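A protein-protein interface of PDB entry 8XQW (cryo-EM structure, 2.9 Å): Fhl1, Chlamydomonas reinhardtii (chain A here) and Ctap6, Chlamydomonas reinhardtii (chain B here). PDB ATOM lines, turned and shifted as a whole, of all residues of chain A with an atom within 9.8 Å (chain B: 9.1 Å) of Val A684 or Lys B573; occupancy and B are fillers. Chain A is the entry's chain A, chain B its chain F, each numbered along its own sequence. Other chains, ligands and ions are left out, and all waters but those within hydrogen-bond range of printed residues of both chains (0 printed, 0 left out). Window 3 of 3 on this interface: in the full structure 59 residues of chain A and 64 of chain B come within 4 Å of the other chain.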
ATOM      1  N   PRO A 648      12.849 -20.360  -3.637  1.00  0.00           N
ATOM      2  CA  PRO A 648      11.618 -19.728  -4.126  1.00  0.00           C
ATOM      3  C   PRO A 648      10.637 -20.774  -4.632  1.00  0.00           C
ATOM      4  O   PRO A 648      10.986 -21.629  -5.449  1.00  0.00           O
ATOM      5  CB  PRO A 648      12.114 -18.827  -5.263  1.00  0.00           C
ATOM      6  CG  PRO A 648      13.311 -19.535  -5.783  1.00  0.00           C
ATOM      7  CD  PRO A 648      13.935 -20.285  -4.627  1.00  0.00           C
ATOM      8  N   ASN A 677      17.693 -29.528  -4.469  1.00  0.00           N
ATOM      9  CA  ASN A 677      18.851 -28.724  -4.945  1.00  0.00           C
ATOM     10  C   ASN A 677      18.780 -28.588  -6.464  1.00  0.00           C
ATOM     11  O   ASN A 677      18.833 -27.452  -6.961  1.00  0.00           O
ATOM     12  CB  ASN A 677      20.180 -29.339  -4.534  1.00  0.00           C
ATOM     13  CG  ASN A 677      21.341 -28.808  -5.338  1.00  0.00           C
ATOM     14  OD1 ASN A 677      21.482 -27.590  -5.490  1.00  0.00           O
ATOM     15  ND2 ASN A 677      22.185 -29.695  -5.840  1.00  0.00           N
ATOM     16  N   GLU A 678      18.654 -29.704  -7.177  1.00  0.00           N
ATOM     17  CA  GLU A 678      18.666 -29.674  -8.663  1.00  0.00           C
ATOM     18  C   GLU A 678      17.568 -28.739  -9.179  1.00  0.00           C
ATOM     19  O   GLU A 678      17.820 -28.013 -10.155  1.00  0.00           O
ATOM     20  CB  GLU A 678      18.493 -31.084  -9.225  1.00  0.00           C
ATOM     21  CG  GLU A 678      19.796 -31.712  -9.709  1.00  0.00           C
ATOM     22  CD  GLU A 678      21.014 -31.472  -8.836  1.00  0.00           C
ATOM     23  OE1 GLU A 678      20.924 -31.682  -7.608  1.00  0.00           O
ATOM     24  OE2 GLU A 678      22.061 -31.087  -9.389  1.00  0.00           O
ATOM     25  N   ALA A 679      16.398 -28.759  -8.549  1.00  0.00           N
ATOM     26  CA  ALA A 679      15.302 -27.867  -8.973  1.00  0.00           C
ATOM     27  C   ALA A 679      15.793 -26.422  -8.960  1.00  0.00           C
ATOM     28  O   ALA A 679      15.555 -25.689  -9.940  1.00  0.00           O
ATOM     29  CB  ALA A 679      14.118 -28.040  -8.063  1.00  0.00           C
ATOM     30  N   ALA A 680      16.452 -26.012  -7.881  1.00  0.00           N
ATOM     31  CA  ALA A 680      16.870 -24.597  -7.784  1.00  0.00           C
ATOM     32  C   ALA A 680      17.890 -24.289  -8.886  1.00  0.00           C
ATOM     33  O   ALA A 680      17.713 -23.278  -9.593  1.00  0.00           O
ATOM     34  CB  ALA A 680      17.394 -24.337  -6.400  1.00  0.00           C
ATOM     35  N   ILE A 681      18.904 -25.140  -9.063  1.00  0.00           N
ATOM     36  CA  ILE A 681      19.872 -24.949 -10.185  1.00  0.00           C
ATOM     37  C   ILE A 681      19.072 -24.750 -11.478  1.00  0.00           C
ATOM     38  O   ILE A 681      19.369 -23.800 -12.226  1.00  0.00           O
ATOM     39  CB  ILE A 681      20.827 -26.150 -10.287  1.00  0.00           C
ATOM     40  CG1 ILE A 681      21.997 -26.016  -9.320  1.00  0.00           C
ATOM     41  CG2 ILE A 681      21.311 -26.372 -11.720  1.00  0.00           C
ATOM     42  CD1 ILE A 681      22.568 -27.344  -8.862  1.00  0.00           C
ATOM     43  N   LEU A 682      18.071 -25.590 -11.706  1.00  0.00           N
ATOM     44  CA  LEU A 682      17.293 -25.503 -12.964  1.00  0.00           C
ATOM     45  C   LEU A 682      16.682 -24.108 -13.081  1.00  0.00           C
ATOM     46  O   LEU A 682      16.908 -23.466 -14.122  1.00  0.00           O
ATOM     47  CB  LEU A 682      16.210 -26.574 -12.987  1.00  0.00           C
ATOM     48  CG  LEU A 682      15.587 -26.859 -14.354  1.00  0.00           C
ATOM     49  CD1 LEU A 682      16.634 -27.464 -15.266  1.00  0.00           C
ATOM     50  CD2 LEU A 682      14.391 -27.785 -14.215  1.00  0.00           C
ATOM     51  N   THR A 683      15.944 -23.655 -12.066  1.00  0.00           N
ATOM     52  CA  THR A 683      15.246 -22.355 -12.206  1.00  0.00           C
ATOM     53  C   THR A 683      16.189 -21.356 -12.830  1.00  0.00           C
ATOM     54  O   THR A 683      15.831 -20.786 -13.885  1.00  0.00           O
ATOM     55  CB  THR A 683      14.695 -21.857 -10.873  1.00  0.00           C
ATOM     56  OG1 THR A 683      15.403 -22.548  -9.854  1.00  0.00           O
ATOM     57  CG2 THR A 683      13.214 -22.147 -10.720  1.00  0.00           C
ATOM     58  N   VAL A 684      17.382 -21.182 -12.257  1.00  0.00           N
ATOM     59  CA  VAL A 684      18.399 -20.265 -12.857  1.00  0.00           C
ATOM     60  C   VAL A 684      18.624 -20.662 -14.321  1.00  0.00           C
ATOM     61  O   VAL A 684      18.231 -19.878 -15.210  1.00  0.00           O
ATOM     62  CB  VAL A 684      19.716 -20.310 -12.059  1.00  0.00           C
ATOM     63  CG1 VAL A 684      20.922 -19.925 -12.905  1.00  0.00           C
ATOM     64  CG2 VAL A 684      19.647 -19.402 -10.843  1.00  0.00           C
ATOM     65  N   ARG A 685      19.189 -21.845 -14.557  1.00  0.00           N
ATOM     66  CA  ARG A 685      19.511 -22.311 -15.929  1.00  0.00           C
ATOM     67  C   ARG A 685      18.456 -21.870 -16.951  1.00  0.00           C
ATOM     68  O   ARG A 685      18.860 -21.506 -18.069  1.00  0.00           O
ATOM     69  CB  ARG A 685      19.615 -23.837 -15.895  1.00  0.00           C
ATOM     70  CG  ARG A 685      19.892 -24.546 -17.211  1.00  0.00           C
ATOM     71  CD  ARG A 685      20.431 -25.936 -16.937  1.00  0.00           C
ATOM     72  NE  ARG A 685      20.228 -26.815 -18.092  1.00  0.00           N
ATOM     73  CZ  ARG A 685      19.207 -27.646 -18.232  1.00  0.00           C
ATOM     74  NH1 ARG A 685      19.233 -28.826 -17.641  1.00  0.00           N
ATOM     75  NH2 ARG A 685      18.166 -27.296 -18.964  1.00  0.00           N
ATOM     76  N   ARG A 686      17.167 -21.897 -16.609  1.00  0.00           N
ATOM     77  CA  ARG A 686      16.145 -21.597 -17.645  1.00  0.00           C
ATOM     78  C   ARG A 686      15.334 -20.325 -17.331  1.00  0.00           C
ATOM     79  O   ARG A 686      14.169 -20.278 -17.779  1.00  0.00           O
ATOM     80  CB  ARG A 686      15.260 -22.835 -17.807  1.00  0.00           C
ATOM     81  CG  ARG A 686      15.880 -24.138 -17.324  1.00  0.00           C
ATOM     82  CD  ARG A 686      15.355 -25.315 -18.125  1.00  0.00           C
ATOM     83  NE  ARG A 686      14.281 -26.034 -17.430  1.00  0.00           N
ATOM     84  CZ  ARG A 686      13.014 -25.643 -17.373  1.00  0.00           C
ATOM     85  NH1 ARG A 686      12.589 -24.910 -16.358  1.00  0.00           N
ATOM     86  NH2 ARG A 686      12.175 -25.989 -18.331  1.00  0.00           N
ATOM     87  N   ASN A 687      15.892 -19.348 -16.602  1.00  0.00           N
ATOM     88  CA  ASN A 687      15.216 -18.027 -16.387  1.00  0.00           C
ATOM     89  C   ASN A 687      13.784 -18.156 -15.863  1.00  0.00           C
ATOM     90  O   ASN A 687      12.865 -17.720 -16.577  1.00  0.00           O
ATOM     91  CB  ASN A 687      15.251 -17.180 -17.652  1.00  0.00           C
ATOM     92  CG  ASN A 687      16.522 -17.402 -18.434  1.00  0.00           C
ATOM     93  OD1 ASN A 687      16.487 -17.983 -19.524  1.00  0.00           O
ATOM     94  ND2 ASN A 687      17.651 -16.969 -17.892  1.00  0.00           N
ATOM     95  N   VAL A 688      13.598 -18.711 -14.669  1.00  0.00           N
ATOM     96  CA  VAL A 688      12.301 -18.854 -14.011  1.00  0.00           C
ATOM     97  C   VAL A 688      12.445 -18.394 -12.565  1.00  0.00           C
ATOM     98  O   VAL A 688      13.430 -18.747 -11.905  1.00  0.00           O
ATOM     99  CB  VAL A 688      11.786 -20.299 -14.091  1.00  0.00           C
ATOM    100  CG1 VAL A 688      10.271 -20.327 -14.003  1.00  0.00           C
ATOM    101  CG2 VAL A 688      12.261 -20.974 -15.370  1.00  0.00           C
ATOM    102  N   PRO A 689      11.509 -17.598 -12.037  1.00  0.00           N
ATOM    103  CA  PRO A 689      11.688 -17.090 -10.665  1.00  0.00           C
ATOM    104  C   PRO A 689      11.685 -18.177  -9.606  1.00  0.00           C
ATOM    105  O   PRO A 689      12.647 -18.300  -8.839  1.00  0.00           O
ATOM    106  CB  PRO A 689      10.503 -16.127 -10.499  1.00  0.00           C
ATOM    107  CG  PRO A 689       9.483 -16.613 -11.471  1.00  0.00           C
ATOM    108  CD  PRO A 689      10.268 -17.099 -12.651  1.00  0.00           C
ATOM    109  N   ALA A 690      10.627 -18.978  -9.548  1.00  0.00           N
ATOM    110  CA  ALA A 690      10.466 -19.991  -8.518  1.00  0.00           C
ATOM    111  C   ALA A 690      10.120 -21.319  -9.174  1.00  0.00           C
ATOM    112  O   ALA A 690       9.865 -21.396 -10.379  1.00  0.00           O
ATOM    113  CB  ALA A 690       9.393 -19.580  -7.504  1.00  0.00           C
ATOM    114  N   ILE A 691      10.108 -22.371  -8.370  1.00  0.00           N
ATOM    115  CA  ILE A 691       9.917 -23.725  -8.868  1.00  0.00           C
ATOM    116  C   ILE A 691       8.428 -24.032  -8.895  1.00  0.00           C
ATOM    117  O   ILE A 691       7.723 -23.829  -7.899  1.00  0.00           O
ATOM    118  CB  ILE A 691      10.677 -24.738  -8.002  1.00  0.00           C
ATOM    119  CG1 ILE A 691      11.938 -24.102  -7.429  1.00  0.00           C
ATOM    120  CG2 ILE A 691      11.077 -25.928  -8.829  1.00  0.00           C
ATOM    121  CD1 ILE A 691      12.564 -24.908  -6.317  1.00  0.00           C
ATOM    122  N   MET A 695       7.729 -28.543 -13.699  1.00  0.00           N
ATOM    123  CA  MET A 695       9.181 -28.679 -13.767  1.00  0.00           C
ATOM    124  C   MET A 695       9.681 -29.734 -12.788  1.00  0.00           C
ATOM    125  O   MET A 695      10.505 -30.583 -13.146  1.00  0.00           O
ATOM    126  CB  MET A 695       9.847 -27.332 -13.505  1.00  0.00           C
ATOM    127  CG  MET A 695       9.135 -26.478 -12.483  1.00  0.00           C
ATOM    128  SD  MET A 695       9.671 -24.757 -12.518  1.00  0.00           S
ATOM    129  CE  MET A 695      11.415 -24.952 -12.880  1.00  0.00           C
ATOM    130  N   MET B 562      28.516 -27.835 -18.127  1.00  0.00           N
ATOM    131  CA  MET B 562      28.703 -26.367 -18.194  1.00  0.00           C
ATOM    132  C   MET B 562      28.229 -25.789 -16.860  1.00  0.00           C
ATOM    133  O   MET B 562      28.990 -25.027 -16.238  1.00  0.00           O
ATOM    134  CB  MET B 562      27.895 -25.757 -19.344  1.00  0.00           C
ATOM    135  CG  MET B 562      27.420 -24.335 -19.104  1.00  0.00           C
ATOM    136  SD  MET B 562      25.711 -24.246 -18.532  1.00  0.00           S
ATOM    137  CE  MET B 562      24.829 -24.461 -20.084  1.00  0.00           C
ATOM    138  N   GLU B 563      27.019 -26.149 -16.440  1.00  0.00           N
ATOM    139  CA  GLU B 563      26.535 -25.686 -15.120  1.00  0.00           C
ATOM    140  C   GLU B 563      27.645 -25.902 -14.096  1.00  0.00           C
ATOM    141  O   GLU B 563      27.850 -24.992 -13.272  1.00  0.00           O
ATOM    142  CB  GLU B 563      25.290 -26.428 -14.634  1.00  0.00           C
ATOM    143  CG  GLU B 563      24.317 -25.534 -13.871  1.00  0.00           C
ATOM    144  CD  GLU B 563      23.487 -24.568 -14.701  1.00  0.00           C
ATOM    145  OE1 GLU B 563      23.533 -24.640 -15.948  1.00  0.00           O
ATOM    146  OE2 GLU B 563      22.782 -23.736 -14.093  1.00  0.00           O
ATOM    147  N   VAL B 564      28.358 -27.034 -14.157  1.00  0.00           N
ATOM    148  CA  VAL B 564      29.335 -27.222 -13.088  1.00  0.00           C
ATOM    149  C   VAL B 564      30.508 -26.263 -13.246  1.00  0.00           C
ATOM    150  O   VAL B 564      31.092 -25.825 -12.252  1.00  0.00           O
ATOM    151  CB  VAL B 564      29.809 -28.688 -13.004  1.00  0.00           C
ATOM    152  CG1 VAL B 564      30.330 -29.171 -14.338  1.00  0.00           C
ATOM    153  CG2 VAL B 564      30.876 -28.842 -11.928  1.00  0.00           C
ATOM    154  N   VAL B 565      30.857 -25.887 -14.477  1.00  0.00           N
ATOM    155  CA  VAL B 565      31.891 -24.871 -14.669  1.00  0.00           C
ATOM    156  C   VAL B 565      31.437 -23.541 -14.082  1.00  0.00           C
ATOM    157  O   VAL B 565      32.173 -22.885 -13.330  1.00  0.00           O
ATOM    158  CB  VAL B 565      32.241 -24.743 -16.164  1.00  0.00           C
ATOM    159  CG1 VAL B 565      32.696 -23.333 -16.490  1.00  0.00           C
ATOM    160  CG2 VAL B 565      33.318 -25.750 -16.547  1.00  0.00           C
ATOM    161  N   ASP B 566      30.210 -23.129 -14.417  1.00  0.00           N
ATOM    162  CA  ASP B 566      29.631 -21.922 -13.839  1.00  0.00           C
ATOM    163  C   ASP B 566      29.647 -21.984 -12.319  1.00  0.00           C
ATOM    164  O   ASP B 566      29.958 -20.997 -11.647  1.00  0.00           O
ATOM    165  CB  ASP B 566      28.202 -21.732 -14.349  1.00  0.00           C
ATOM    166  CG  ASP B 566      28.145 -21.012 -15.683  1.00  0.00           C
ATOM    167  OD1 ASP B 566      28.334 -21.674 -16.721  1.00  0.00           O
ATOM    168  OD2 ASP B 566      27.901 -19.787 -15.696  1.00  0.00           O
ATOM    169  N   PHE B 567      29.320 -23.143 -11.757  1.00  0.00           N
ATOM    170  CA  PHE B 567      29.275 -23.253 -10.305  1.00  0.00           C
ATOM    171  C   PHE B 567      30.669 -23.271  -9.697  1.00  0.00           C
ATOM    172  O   PHE B 567      30.836 -22.930  -8.522  1.00  0.00           O
ATOM    173  CB  PHE B 567      28.510 -24.508  -9.897  1.00  0.00           C
ATOM    174  CG  PHE B 567      27.521 -24.273  -8.804  1.00  0.00           C
ATOM    175  CD1 PHE B 567      27.865 -23.521  -7.697  1.00  0.00           C
ATOM    176  CD2 PHE B 567      26.241 -24.793  -8.887  1.00  0.00           C
ATOM    177  CE1 PHE B 567      26.958 -23.295  -6.692  1.00  0.00           C
ATOM    178  CE2 PHE B 567      25.330 -24.570  -7.885  1.00  0.00           C
ATOM    179  CZ  PHE B 567      25.687 -23.821  -6.786  1.00  0.00           C
ATOM    180  N   THR B 570      32.924 -19.321 -11.358  1.00  0.00           N
ATOM    181  CA  THR B 570      32.203 -18.056 -11.261  1.00  0.00           C
ATOM    182  C   THR B 570      30.838 -18.300 -10.629  1.00  0.00           C
ATOM    183  O   THR B 570      29.828 -18.396 -11.337  1.00  0.00           O
ATOM    184  CB  THR B 570      32.042 -17.401 -12.633  1.00  0.00           C
ATOM    185  OG1 THR B 570      31.079 -18.133 -13.402  1.00  0.00           O
ATOM    186  CG2 THR B 570      33.363 -17.384 -13.382  1.00  0.00           C
ATOM    187  N   PRO B 571      30.763 -18.370  -9.307  1.00  0.00           N
ATOM    188  CA  PRO B 571      29.451 -18.577  -8.652  1.00  0.00           C
ATOM    189  C   PRO B 571      28.570 -17.336  -8.767  1.00  0.00           C
ATOM    190  O   PRO B 571      28.437 -16.520  -7.859  1.00  0.00           O
ATOM    191  CB  PRO B 571      29.843 -18.887  -7.206  1.00  0.00           C
ATOM    192  CG  PRO B 571      31.157 -18.231  -7.019  1.00  0.00           C
ATOM    193  CD  PRO B 571      31.867 -18.333  -8.336  1.00  0.00           C
ATOM    194  N   GLU B 572      27.935 -17.201  -9.932  1.00  0.00           N
ATOM    195  CA  GLU B 572      27.241 -15.974 -10.323  1.00  0.00           C
ATOM    196  C   GLU B 572      25.901 -15.790  -9.613  1.00  0.00           C
ATOM    197  O   GLU B 572      25.719 -14.833  -8.853  1.00  0.00           O
ATOM    198  CB  GLU B 572      27.000 -15.968 -11.838  1.00  0.00           C
ATOM    199  CG  GLU B 572      28.202 -16.249 -12.711  1.00  0.00           C
ATOM    200  CD  GLU B 572      27.896 -16.040 -14.181  1.00  0.00           C
ATOM    201  OE1 GLU B 572      27.871 -17.037 -14.930  1.00  0.00           O
ATOM    202  OE2 GLU B 572      27.662 -14.885 -14.588  1.00  0.00           O
ATOM    203  N   LYS B 573      24.958 -16.700  -9.854  1.00  0.00           N
ATOM    204  CA  LYS B 573      23.559 -16.464  -9.520  1.00  0.00           C
ATOM    205  C   LYS B 573      23.028 -17.434  -8.481  1.00  0.00           C
ATOM    206  O   LYS B 573      21.935 -17.223  -7.938  1.00  0.00           O
ATOM    207  CB  LYS B 573      22.708 -16.576 -10.786  1.00  0.00           C
ATOM    208  CG  LYS B 573      23.326 -15.887 -11.985  1.00  0.00           C
ATOM    209  CD  LYS B 573      23.365 -16.792 -13.210  1.00  0.00           C
ATOM    210  CE  LYS B 573      24.366 -17.926 -13.051  1.00  0.00           C
ATOM    211  NZ  LYS B 573      24.157 -18.996 -14.064  1.00  0.00           N
ATOM    212  N   PHE B 574      23.777 -18.492  -8.191  1.00  0.00           N
ATOM    213  CA  PHE B 574      23.293 -19.562  -7.335  1.00  0.00           C
ATOM    214  C   PHE B 574      23.126 -19.145  -5.881  1.00  0.00           C
ATOM    215  O   PHE B 574      22.621 -19.945  -5.087  1.00  0.00           O
ATOM    216  CB  PHE B 574      24.230 -20.759  -7.463  1.00  0.00           C
ATOM    217  CG  PHE B 574      24.349 -21.263  -8.872  1.00  0.00           C
ATOM    218  CD1 PHE B 574      23.217 -21.479  -9.635  1.00  0.00           C
ATOM    219  CD2 PHE B 574      25.585 -21.496  -9.441  1.00  0.00           C
ATOM    220  CE1 PHE B 574      23.316 -21.933 -10.932  1.00  0.00           C
ATOM    221  CE2 PHE B 574      25.685 -21.949 -10.741  1.00  0.00           C
ATOM    222  CZ  PHE B 574      24.548 -22.166 -11.485  1.00  0.00           C
ATOM    223  N   LYS B 575      23.517 -17.928  -5.504  1.00  0.00           N
ATOM    224  CA  LYS B 575      23.137 -17.419  -4.192  1.00  0.00           C
ATOM    225  C   LYS B 575      21.711 -16.886  -4.220  1.00  0.00           C
ATOM    226  O   LYS B 575      20.942 -17.091  -3.275  1.00  0.00           O
ATOM    227  CB  LYS B 575      24.108 -16.330  -3.730  1.00  0.00           C
ATOM    228  CG  LYS B 575      25.568 -16.760  -3.618  1.00  0.00           C
ATOM    229  CD  LYS B 575      26.316 -16.611  -4.934  1.00  0.00           C
ATOM    230  CE  LYS B 575      27.678 -17.280  -4.872  1.00  0.00           C
ATOM    231  NZ  LYS B 575      27.625 -18.611  -4.202  1.00  0.00           N
ATOM    232  N   ALA B 576      21.347 -16.192  -5.298  1.00  0.00           N
ATOM    233  CA  ALA B 576      19.969 -15.765  -5.494  1.00  0.00           C
ATOM    234  C   ALA B 576      19.037 -16.933  -5.773  1.00  0.00           C
ATOM    235  O   ALA B 576      17.864 -16.876  -5.390  1.00  0.00           O
ATOM    236  CB  ALA B 576      19.890 -14.752  -6.637  1.00  0.00           C
ATOM    237  N   SER B 577      19.528 -17.982  -6.435  1.00  0.00           N
ATOM    238  CA  SER B 577      18.735 -19.194  -6.595  1.00  0.00           C
ATOM    239  C   SER B 577      18.528 -19.893  -5.258  1.00  0.00           C
ATOM    240  O   SER B 577      17.413 -20.310  -4.924  1.00  0.00           O
ATOM    241  CB  SER B 577      19.417 -20.139  -7.579  1.00  0.00           C
ATOM    242  OG  SER B 577      20.132 -21.147  -6.891  1.00  0.00           O
ATOM    243  N   GLY B 578      19.594 -20.024  -4.480  1.00  0.00           N
ATOM    244  CA  GLY B 578      19.553 -20.778  -3.247  1.00  0.00           C
ATOM    245  C   GLY B 578      20.099 -22.177  -3.358  1.00  0.00           C
ATOM    246  O   GLY B 578      19.941 -22.963  -2.420  1.00  0.00           O
ATOM    247  N   ALA B 579      20.750 -22.510  -4.467  1.00  0.00           N
ATOM    248  CA  ALA B 579      21.155 -23.872  -4.765  1.00  0.00           C
ATOM    249  C   ALA B 579      22.587 -24.122  -4.320  1.00  0.00           C
ATOM    250  O   ALA B 579      23.486 -23.307  -4.541  1.00  0.00           O
ATOM    251  CB  ALA B 579      21.019 -24.165  -6.261  1.00  0.00           C
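O of Pro A648 sits at hydrogen-bond distance from N of Ile A691 (3.1 Å). ND2 of Asn A677 lies within hydrogen-bond range of OE1 of Glu A678 (2.9 Å). O of Ala A680 sits at hydrogen-bond distance from OG1 of Thr A683 (2.4 Å). The backbone carbonyl oxygen of Phe B574 lies within hydrogen-bond range of the side-chain hydroxyl of Ser B577 (3.3 Å). N of Ala B579 sits at hydrogen-bond distance from O of Phe B574 (3.2 Å). The side-chain hydroxyl (OG) of Ser B577 lies within hydrogen-bond range of the backbone NH (N) of Ala B579 (2.8 Å).
Hydrophobic or aromatic side chains of chain B within 4 Å of the printed part of chain A: Phe B567, Phe B574 and Ala B579. Hydrophobic or aromatic side chains of chain A within 4 Å of the printed part of chain B: Pro A648, Ala A680, Ile A681 and Val A684. Among the printed residues, no Asp or Glu carboxylate lies within 4 Å of a Lys or Arg side-chain nitrogen of the other chain.
Among the printed residues, merely in contact across the chains: Val A684 with Ser B577 (3.4 Å), Pro A648 with Ser B577 (3.5 Å), Arg A685 with Glu B563 (3.5 Å), Asn A677 with Ala B579 (3.5 Å), Val A684 with Lys B573 (3.6 Å), Ala A680 with Ala B579 (3.6 Å), Ile A681 with Ala B579 (3.6 Å), Val A684 with Phe B574 (3.7 Å), Ile A681 with Glu B563 (3.8 Å) and Ile A681 with Phe B567 (3.9 Å).
Of chain B, only Lys B573, Phe B574 and Ser B577 come within 4 Å of Val A684. Printed residues of chain A within 4 Å of Glu B563: Ile A681 and Arg A685. Of the printed residues of chain A, Phe B567 touches Ile A681 (3.9 Å). No residue of chain A comes within 4 Å of Glu B572. Lys B573 touches one residue of chain A. Of the printed residues of chain A, Ser B577 touches Pro A648 and Val A684. The nearest printed residue of chain A that does not touch Ser B577 is Ala A680 (4.1 Å).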
